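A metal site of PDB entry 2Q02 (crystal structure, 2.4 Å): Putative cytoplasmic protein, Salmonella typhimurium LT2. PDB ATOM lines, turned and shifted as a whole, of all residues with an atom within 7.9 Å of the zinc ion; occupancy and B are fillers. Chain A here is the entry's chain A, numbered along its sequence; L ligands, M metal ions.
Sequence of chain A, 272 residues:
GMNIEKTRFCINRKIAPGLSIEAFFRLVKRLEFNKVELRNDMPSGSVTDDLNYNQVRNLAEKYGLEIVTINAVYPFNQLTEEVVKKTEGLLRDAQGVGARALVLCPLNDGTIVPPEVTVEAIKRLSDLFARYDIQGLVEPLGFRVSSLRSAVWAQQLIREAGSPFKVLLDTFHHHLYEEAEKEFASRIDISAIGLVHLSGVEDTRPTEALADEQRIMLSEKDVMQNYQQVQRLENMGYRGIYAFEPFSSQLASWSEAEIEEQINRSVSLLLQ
OD1 of Asp 170 lies within salt-bridge range of NH2 of Arg 215 (3.3 Å). OD1 of Asp 170 is in hydrogen-bond range of N of Phe 172, 3.1 Å away. The guanidinium group (NH2) of Arg 215 sits at hydrogen-bond distance from the backbone carbonyl oxygen (O) of Glu 245 (3.2 Å). The side-chain carboxylate of Glu 245 is in salt-bridge range of the guanidinium group of Arg 39, 2.9 Å away. O of Leu 198 sits at hydrogen-bond distance from N of Glu 245 (2.7 Å). The backbone carbonyl oxygen (O) of Leu 169 lies within hydrogen-bond range of the backbone NH (N) of His 197. The backbone NH (N) of Thr 171 lies within hydrogen-bond range of the backbone carbonyl oxygen (O) of His 197 (2.9 Å). NE2 of His 197 sits at hydrogen-bond distance from OE2 of Glu 37 (3.0 Å).
Within 4 Å of the zinc ion: Glu 139, Asp 170, His 197 and Glu 245.
The zinc ion is bound by the side-chain carboxylate (OD2) of Asp 170, the side-chain carboxylate (OE2) of Glu 139, the side-chain carboxylate (OE1) of Glu 245, a ring nitrogen (ND1) of His 197 and an oxygen (O1) of the ligand.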
ATOM      1  N   ASN A  12     -28.903  10.058   9.940  1.00  0.00           N
ATOM      2  CA  ASN A  12     -27.828   9.099  10.109  1.00  0.00           C
ATOM      3  C   ASN A  12     -27.961   8.428  11.511  1.00  0.00           C
ATOM      4  O   ASN A  12     -28.240   9.093  12.524  1.00  0.00           O
ATOM      5  CB  ASN A  12     -26.471   9.807   9.924  1.00  0.00           C
ATOM      6  CG  ASN A  12     -25.318   8.836   9.814  1.00  0.00           C
ATOM      7  OD1 ASN A  12     -25.096   8.029  10.718  1.00  0.00           O
ATOM      8  ND2 ASN A  12     -24.552   8.918   8.711  1.00  0.00           N
ATOM      9  N   GLU A  37     -29.462   6.440   7.241  1.00  0.00           N
ATOM     10  CA  GLU A  37     -28.212   5.788   6.931  1.00  0.00           C
ATOM     11  C   GLU A  37     -27.918   4.797   8.041  1.00  0.00           C
ATOM     12  O   GLU A  37     -28.080   5.118   9.230  1.00  0.00           O
ATOM     13  CB  GLU A  37     -27.062   6.803   6.909  1.00  0.00           C
ATOM     14  CG  GLU A  37     -27.132   7.851   5.810  1.00  0.00           C
ATOM     15  CD  GLU A  37     -25.916   8.761   5.812  1.00  0.00           C
ATOM     16  OE1 GLU A  37     -25.966   9.795   6.541  1.00  0.00           O
ATOM     17  OE2 GLU A  37     -24.898   8.416   5.127  1.00  0.00           O
ATOM     18  N   ARG A  39     -24.826   1.966   9.630  1.00  0.00           N
ATOM     19  CA  ARG A  39     -23.395   2.079   9.897  1.00  0.00           C
ATOM     20  C   ARG A  39     -22.756   0.805  10.512  1.00  0.00           C
ATOM     21  O   ARG A  39     -23.377   0.092  11.327  1.00  0.00           O
ATOM     22  CB  ARG A  39     -23.121   3.232  10.863  1.00  0.00           C
ATOM     23  CG  ARG A  39     -23.890   4.550  10.636  1.00  0.00           C
ATOM     24  CD  ARG A  39     -23.452   5.557  11.703  1.00  0.00           C
ATOM     25  NE  ARG A  39     -21.999   5.689  11.672  1.00  0.00           N
ATOM     26  CZ  ARG A  39     -21.333   6.583  10.942  1.00  0.00           C
ATOM     27  NH1 ARG A  39     -21.955   7.501  10.222  1.00  0.00           N
ATOM     28  NH2 ARG A  39     -20.021   6.580  10.962  1.00  0.00           N
ATOM     29  N   ASN A  71     -22.350   3.540   6.102  1.00  0.00           N
ATOM     30  CA  ASN A  71     -21.039   4.085   6.484  1.00  0.00           C
ATOM     31  C   ASN A  71     -20.294   3.025   7.269  1.00  0.00           C
ATOM     32  O   ASN A  71     -20.814   2.585   8.301  1.00  0.00           O
ATOM     33  CB  ASN A  71     -21.191   5.289   7.427  1.00  0.00           C
ATOM     34  CG  ASN A  71     -21.794   6.494   6.759  1.00  0.00           C
ATOM     35  OD1 ASN A  71     -21.074   7.439   6.429  1.00  0.00           O
ATOM     36  ND2 ASN A  71     -23.143   6.499   6.571  1.00  0.00           N
ATOM     37  N   VAL A 103     -20.441   4.272   1.571  1.00  0.00           N
ATOM     38  CA  VAL A 103     -19.508   5.385   1.741  1.00  0.00           C
ATOM     39  C   VAL A 103     -18.064   4.905   1.824  1.00  0.00           C
ATOM     40  O   VAL A 103     -17.755   3.911   2.503  1.00  0.00           O
ATOM     41  CB  VAL A 103     -19.829   6.179   3.018  1.00  0.00           C
ATOM     42  CG1 VAL A 103     -18.785   7.277   3.255  1.00  0.00           C
ATOM     43  CG2 VAL A 103     -21.213   6.780   2.945  1.00  0.00           C
ATOM     44  N   CYS A 105     -14.058   6.092   2.710  1.00  0.00           N
ATOM     45  CA  CYS A 105     -13.243   7.056   3.417  1.00  0.00           C
ATOM     46  C   CYS A 105     -11.774   6.819   3.183  1.00  0.00           C
ATOM     47  O   CYS A 105     -11.310   5.666   3.270  1.00  0.00           O
ATOM     48  CB  CYS A 105     -13.492   6.967   4.922  1.00  0.00           C
ATOM     49  SG  CYS A 105     -15.104   7.619   5.429  1.00  0.00           S
ATOM     50  N   GLU A 139     -15.952  10.210   0.486  1.00  0.00           N
ATOM     51  CA  GLU A 139     -16.017  11.291   1.472  1.00  0.00           C
ATOM     52  C   GLU A 139     -14.612  11.743   1.868  1.00  0.00           C
ATOM     53  O   GLU A 139     -13.951  11.056   2.647  1.00  0.00           O
ATOM     54  CB  GLU A 139     -16.707  10.836   2.751  1.00  0.00           C
ATOM     55  CG  GLU A 139     -16.737  11.899   3.854  1.00  0.00           C
ATOM     56  CD  GLU A 139     -17.751  11.598   4.928  1.00  0.00           C
ATOM     57  OE1 GLU A 139     -18.108  10.415   5.085  1.00  0.00           O
ATOM     58  OE2 GLU A 139     -18.191  12.541   5.614  1.00  0.00           O
ATOM     59  N   PRO A 140     -14.166  12.882   1.333  1.00  0.00           N
ATOM     60  CA  PRO A 140     -12.941  13.475   1.846  1.00  0.00           C
ATOM     61  C   PRO A 140     -13.033  13.820   3.347  1.00  0.00           C
ATOM     62  O   PRO A 140     -14.096  14.267   3.844  1.00  0.00           O
ATOM     63  CB  PRO A 140     -12.787  14.768   1.032  1.00  0.00           C
ATOM     64  CG  PRO A 140     -13.672  14.655  -0.138  1.00  0.00           C
ATOM     65  CD  PRO A 140     -14.735  13.641   0.204  1.00  0.00           C
ATOM     66  N   LEU A 141     -11.918  13.594   4.049  1.00  0.00           N
ATOM     67  CA  LEU A 141     -11.774  13.923   5.460  1.00  0.00           C
ATOM     68  C   LEU A 141     -10.856  15.109   5.568  1.00  0.00           C
ATOM     69  O   LEU A 141      -9.766  15.109   5.010  1.00  0.00           O
ATOM     70  CB  LEU A 141     -11.177  12.776   6.244  1.00  0.00           C
ATOM     71  CG  LEU A 141     -11.827  11.412   6.056  1.00  0.00           C
ATOM     72  CD1 LEU A 141     -11.001  10.370   6.735  1.00  0.00           C
ATOM     73  CD2 LEU A 141     -13.245  11.399   6.578  1.00  0.00           C
ATOM     74  N   LEU A 168     -19.161  12.798  -1.277  1.00  0.00           N
ATOM     75  CA  LEU A 168     -19.954  13.039  -0.097  1.00  0.00           C
ATOM     76  C   LEU A 168     -19.371  14.283   0.624  1.00  0.00           C
ATOM     77  O   LEU A 168     -18.256  14.240   1.177  1.00  0.00           O
ATOM     78  CB  LEU A 168     -19.916  11.812   0.805  1.00  0.00           C
ATOM     79  CG  LEU A 168     -20.994  11.741   1.861  1.00  0.00           C
ATOM     80  CD1 LEU A 168     -20.869  10.396   2.621  1.00  0.00           C
ATOM     81  CD2 LEU A 168     -20.979  12.975   2.812  1.00  0.00           C
ATOM     82  N   LEU A 169     -20.115  15.379   0.567  1.00  0.00           N
ATOM     83  CA  LEU A 169     -19.668  16.615   1.167  1.00  0.00           C
ATOM     84  C   LEU A 169     -20.121  16.642   2.640  1.00  0.00           C
ATOM     85  O   LEU A 169     -21.300  16.682   2.952  1.00  0.00           O
ATOM     86  CB  LEU A 169     -20.223  17.798   0.361  1.00  0.00           C
ATOM     87  CG  LEU A 169     -19.542  19.166   0.500  1.00  0.00           C
ATOM     88  CD1 LEU A 169     -20.270  20.127  -0.409  1.00  0.00           C
ATOM     89  CD2 LEU A 169     -19.504  19.691   1.937  1.00  0.00           C
ATOM     90  N   ASP A 170     -19.159  16.639   3.531  1.00  0.00           N
ATOM     91  CA  ASP A 170     -19.432  16.705   4.949  1.00  0.00           C
ATOM     92  C   ASP A 170     -19.003  18.096   5.494  1.00  0.00           C
ATOM     93  O   ASP A 170     -17.837  18.478   5.379  1.00  0.00           O
ATOM     94  CB  ASP A 170     -18.660  15.573   5.590  1.00  0.00           C
ATOM     95  CG  ASP A 170     -18.981  15.396   7.021  1.00  0.00           C
ATOM     96  OD1 ASP A 170     -18.894  16.402   7.751  1.00  0.00           O
ATOM     97  OD2 ASP A 170     -19.290  14.256   7.402  1.00  0.00           O
ATOM     98  N   THR A 171     -19.960  18.857   6.042  1.00  0.00           N
ATOM     99  CA  THR A 171     -19.684  20.259   6.411  1.00  0.00           C
ATOM    100  C   THR A 171     -18.548  20.402   7.438  1.00  0.00           C
ATOM    101  O   THR A 171     -17.829  21.398   7.419  1.00  0.00           O
ATOM    102  CB  THR A 171     -20.902  20.974   6.983  1.00  0.00           C
ATOM    103  OG1 THR A 171     -21.384  20.241   8.108  1.00  0.00           O
ATOM    104  CG2 THR A 171     -21.996  21.124   5.916  1.00  0.00           C
ATOM    105  N   PHE A 172     -18.398  19.427   8.322  1.00  0.00           N
ATOM    106  CA  PHE A 172     -17.289  19.401   9.259  1.00  0.00           C
ATOM    107  C   PHE A 172     -15.953  19.241   8.532  1.00  0.00           C
ATOM    108  O   PHE A 172     -14.970  19.942   8.842  1.00  0.00           O
ATOM    109  CB  PHE A 172     -17.462  18.243  10.246  1.00  0.00           C
ATOM    110  CG  PHE A 172     -16.254  17.983  11.112  1.00  0.00           C
ATOM    111  CD1 PHE A 172     -15.272  17.091  10.706  1.00  0.00           C
ATOM    112  CD2 PHE A 172     -16.132  18.582  12.367  1.00  0.00           C
ATOM    113  CE1 PHE A 172     -14.168  16.825  11.541  1.00  0.00           C
ATOM    114  CE2 PHE A 172     -15.050  18.316  13.202  1.00  0.00           C
ATOM    115  CZ  PHE A 172     -14.068  17.425  12.796  1.00  0.00           C
ATOM    116  N   HIS A 173     -15.929  18.309   7.583  1.00  0.00           N
ATOM    117  CA  HIS A 173     -14.693  18.038   6.858  1.00  0.00           C
ATOM    118  C   HIS A 173     -14.314  19.188   5.927  1.00  0.00           C
ATOM    119  O   HIS A 173     -13.134  19.496   5.779  1.00  0.00           O
ATOM    120  CB  HIS A 173     -14.709  16.667   6.179  1.00  0.00           C
ATOM    121  CG  HIS A 173     -14.719  15.543   7.164  1.00  0.00           C
ATOM    122  ND1 HIS A 173     -13.674  15.318   8.044  1.00  0.00           N
ATOM    123  CD2 HIS A 173     -15.657  14.610   7.458  1.00  0.00           C
ATOM    124  CE1 HIS A 173     -13.972  14.275   8.817  1.00  0.00           C
ATOM    125  NE2 HIS A 173     -15.161  13.826   8.476  1.00  0.00           N
ATOM    126  N   LEU A 195     -24.211  13.369  -1.737  1.00  0.00           N
ATOM    127  CA  LEU A 195     -24.844  13.490  -0.433  1.00  0.00           C
ATOM    128  C   LEU A 195     -24.136  14.553   0.374  1.00  0.00           C
ATOM    129  O   LEU A 195     -22.966  14.855   0.112  1.00  0.00           O
ATOM    130  CB  LEU A 195     -24.762  12.170   0.287  1.00  0.00           C
ATOM    131  CG  LEU A 195     -25.341  12.041   1.677  1.00  0.00           C
ATOM    132  CD1 LEU A 195     -26.805  12.228   1.633  1.00  0.00           C
ATOM    133  CD2 LEU A 195     -24.995  10.643   2.235  1.00  0.00           C
ATOM    134  N   VAL A 196     -24.845  15.141   1.335  1.00  0.00           N
ATOM    135  CA  VAL A 196     -24.240  16.102   2.254  1.00  0.00           C
ATOM    136  C   VAL A 196     -24.485  15.656   3.696  1.00  0.00           C
ATOM    137  O   VAL A 196     -25.598  15.244   4.032  1.00  0.00           O
ATOM    138  CB  VAL A 196     -24.761  17.550   2.038  1.00  0.00           C
ATOM    139  CG1 VAL A 196     -24.165  18.493   3.050  1.00  0.00           C
ATOM    140  CG2 VAL A 196     -24.455  18.021   0.609  1.00  0.00           C
ATOM    141  N   HIS A 197     -23.423  15.704   4.506  1.00  0.00           N
ATOM    142  CA  HIS A 197     -23.461  15.372   5.915  1.00  0.00           C
ATOM    143  C   HIS A 197     -23.350  16.664   6.730  1.00  0.00           C
ATOM    144  O   HIS A 197     -22.387  17.439   6.570  1.00  0.00           O
ATOM    145  CB  HIS A 197     -22.312  14.442   6.314  1.00  0.00           C
ATOM    146  CG  HIS A 197     -22.560  12.981   6.063  1.00  0.00           C
ATOM    147  ND1 HIS A 197     -21.615  12.015   6.308  1.00  0.00           N
ATOM    148  CD2 HIS A 197     -23.644  12.321   5.574  1.00  0.00           C
ATOM    149  CE1 HIS A 197     -22.099  10.829   5.990  1.00  0.00           C
ATOM    150  NE2 HIS A 197     -23.325  10.985   5.532  1.00  0.00           N
ATOM    151  N   LEU A 198     -24.342  16.885   7.606  1.00  0.00           N
ATOM    152  CA  LEU A 198     -24.442  18.089   8.405  1.00  0.00           C
ATOM    153  C   LEU A 198     -24.255  17.685   9.874  1.00  0.00           C
ATOM    154  O   LEU A 198     -24.651  16.583  10.314  1.00  0.00           O
ATOM    155  CB  LEU A 198     -25.808  18.768   8.244  1.00  0.00           C
ATOM    156  CG  LEU A 198     -26.316  19.197   6.853  1.00  0.00           C
ATOM    157  CD1 LEU A 198     -27.775  19.722   6.933  1.00  0.00           C
ATOM    158  CD2 LEU A 198     -25.404  20.239   6.246  1.00  0.00           C
ATOM    159  N   SER A 199     -23.596  18.589  10.594  1.00  0.00           N
ATOM    160  CA  SER A 199     -23.433  18.510  12.032  1.00  0.00           C
ATOM    161  C   SER A 199     -22.859  19.846  12.426  1.00  0.00           C
ATOM    162  O   SER A 199     -22.258  20.546  11.592  1.00  0.00           O
ATOM    163  CB  SER A 199     -22.523  17.361  12.468  1.00  0.00           C
ATOM    164  OG  SER A 199     -21.170  17.721  12.461  1.00  0.00           O
ATOM    165  N   ASP A 212     -14.000  14.465  15.690  1.00  0.00           N
ATOM    166  CA  ASP A 212     -15.398  14.029  15.612  1.00  0.00           C
ATOM    167  C   ASP A 212     -16.158  14.116  16.946  1.00  0.00           C
ATOM    168  O   ASP A 212     -17.369  14.347  16.952  1.00  0.00           O
ATOM    169  CB  ASP A 212     -15.497  12.614  15.054  1.00  0.00           C
ATOM    170  CG  ASP A 212     -15.113  12.527  13.585  1.00  0.00           C
ATOM    171  OD1 ASP A 212     -15.202  13.537  12.881  1.00  0.00           O
ATOM    172  OD2 ASP A 212     -14.701  11.448  13.138  1.00  0.00           O
ATOM    173  N   ARG A 215     -18.596  16.971  17.424  1.00  0.00           N
ATOM    174  CA  ARG A 215     -19.649  17.124  16.443  1.00  0.00           C
ATOM    175  C   ARG A 215     -20.986  16.770  17.066  1.00  0.00           C
ATOM    176  O   ARG A 215     -21.273  15.610  17.372  1.00  0.00           O
ATOM    177  CB  ARG A 215     -19.381  16.267  15.206  1.00  0.00           C
ATOM    178  CG  ARG A 215     -18.220  16.772  14.360  1.00  0.00           C
ATOM    179  CD  ARG A 215     -17.842  15.784  13.327  1.00  0.00           C
ATOM    180  NE  ARG A 215     -18.894  15.609  12.352  1.00  0.00           N
ATOM    181  CZ  ARG A 215     -18.815  14.803  11.288  1.00  0.00           C
ATOM    182  NH1 ARG A 215     -17.707  14.087  11.041  1.00  0.00           N
ATOM    183  NH2 ARG A 215     -19.849  14.717  10.462  1.00  0.00           N
ATOM    184  N   ALA A 243     -28.198  14.929   5.256  1.00  0.00           N
ATOM    185  CA  ALA A 243     -28.238  13.906   6.292  1.00  0.00           C
ATOM    186  C   ALA A 243     -27.511  14.436   7.495  1.00  0.00           C
ATOM    187  O   ALA A 243     -26.411  14.934   7.359  1.00  0.00           O
ATOM    188  CB  ALA A 243     -27.541  12.622   5.817  1.00  0.00           C
ATOM    189  N   GLU A 245     -25.434  13.992  10.787  1.00  0.00           N
ATOM    190  CA  GLU A 245     -24.421  13.020  11.242  1.00  0.00           C
ATOM    191  C   GLU A 245     -23.559  13.566  12.406  1.00  0.00           C
ATOM    192  O   GLU A 245     -22.401  13.892  12.240  1.00  0.00           O
ATOM    193  CB  GLU A 245     -23.532  12.556  10.055  1.00  0.00           C
ATOM    194  CG  GLU A 245     -22.547  11.414  10.419  1.00  0.00           C
ATOM    195  CD  GLU A 245     -21.425  11.201   9.397  1.00  0.00           C
ATOM    196  OE1 GLU A 245     -20.878  12.202   8.881  1.00  0.00           O
ATOM    197  OE2 GLU A 245     -21.061  10.043   9.112  1.00  0.00           O
ATOM    198  N   PHE A 247     -21.466  12.965  16.000  1.00  0.00           N
ATOM    199  CA  PHE A 247     -20.575  11.892  16.530  1.00  0.00           C
ATOM    200  C   PHE A 247     -20.303  11.917  18.053  1.00  0.00           C
ATOM    201  O   PHE A 247     -19.824  10.928  18.623  1.00  0.00           O
ATOM    202  CB  PHE A 247     -19.203  11.985  15.859  1.00  0.00           C
ATOM    203  CG  PHE A 247     -19.098  11.264  14.587  1.00  0.00           C
ATOM    204  CD1 PHE A 247     -18.743   9.918  14.571  1.00  0.00           C
ATOM    205  CD2 PHE A 247     -19.319  11.926  13.375  1.00  0.00           C
ATOM    206  CE1 PHE A 247     -18.632   9.228  13.365  1.00  0.00           C
ATOM    207  CE2 PHE A 247     -19.199  11.246  12.168  1.00  0.00           C
ATOM    208  CZ  PHE A 247     -18.857   9.896  12.170  1.00  0.00           C
HETATM  209  O1  LIG L   1     -18.042  11.117   8.681  1.00  0.00           O
HETATM  210  O2  LIG L   1     -16.552  11.474   9.400  1.00  0.00           O
HETATM  211  O3  LIG L   1     -14.155  11.073  10.442  1.00  0.00           O
HETATM  212 ZN    ZN M   1     -19.663  12.358   7.127  1.00  0.00          ZN
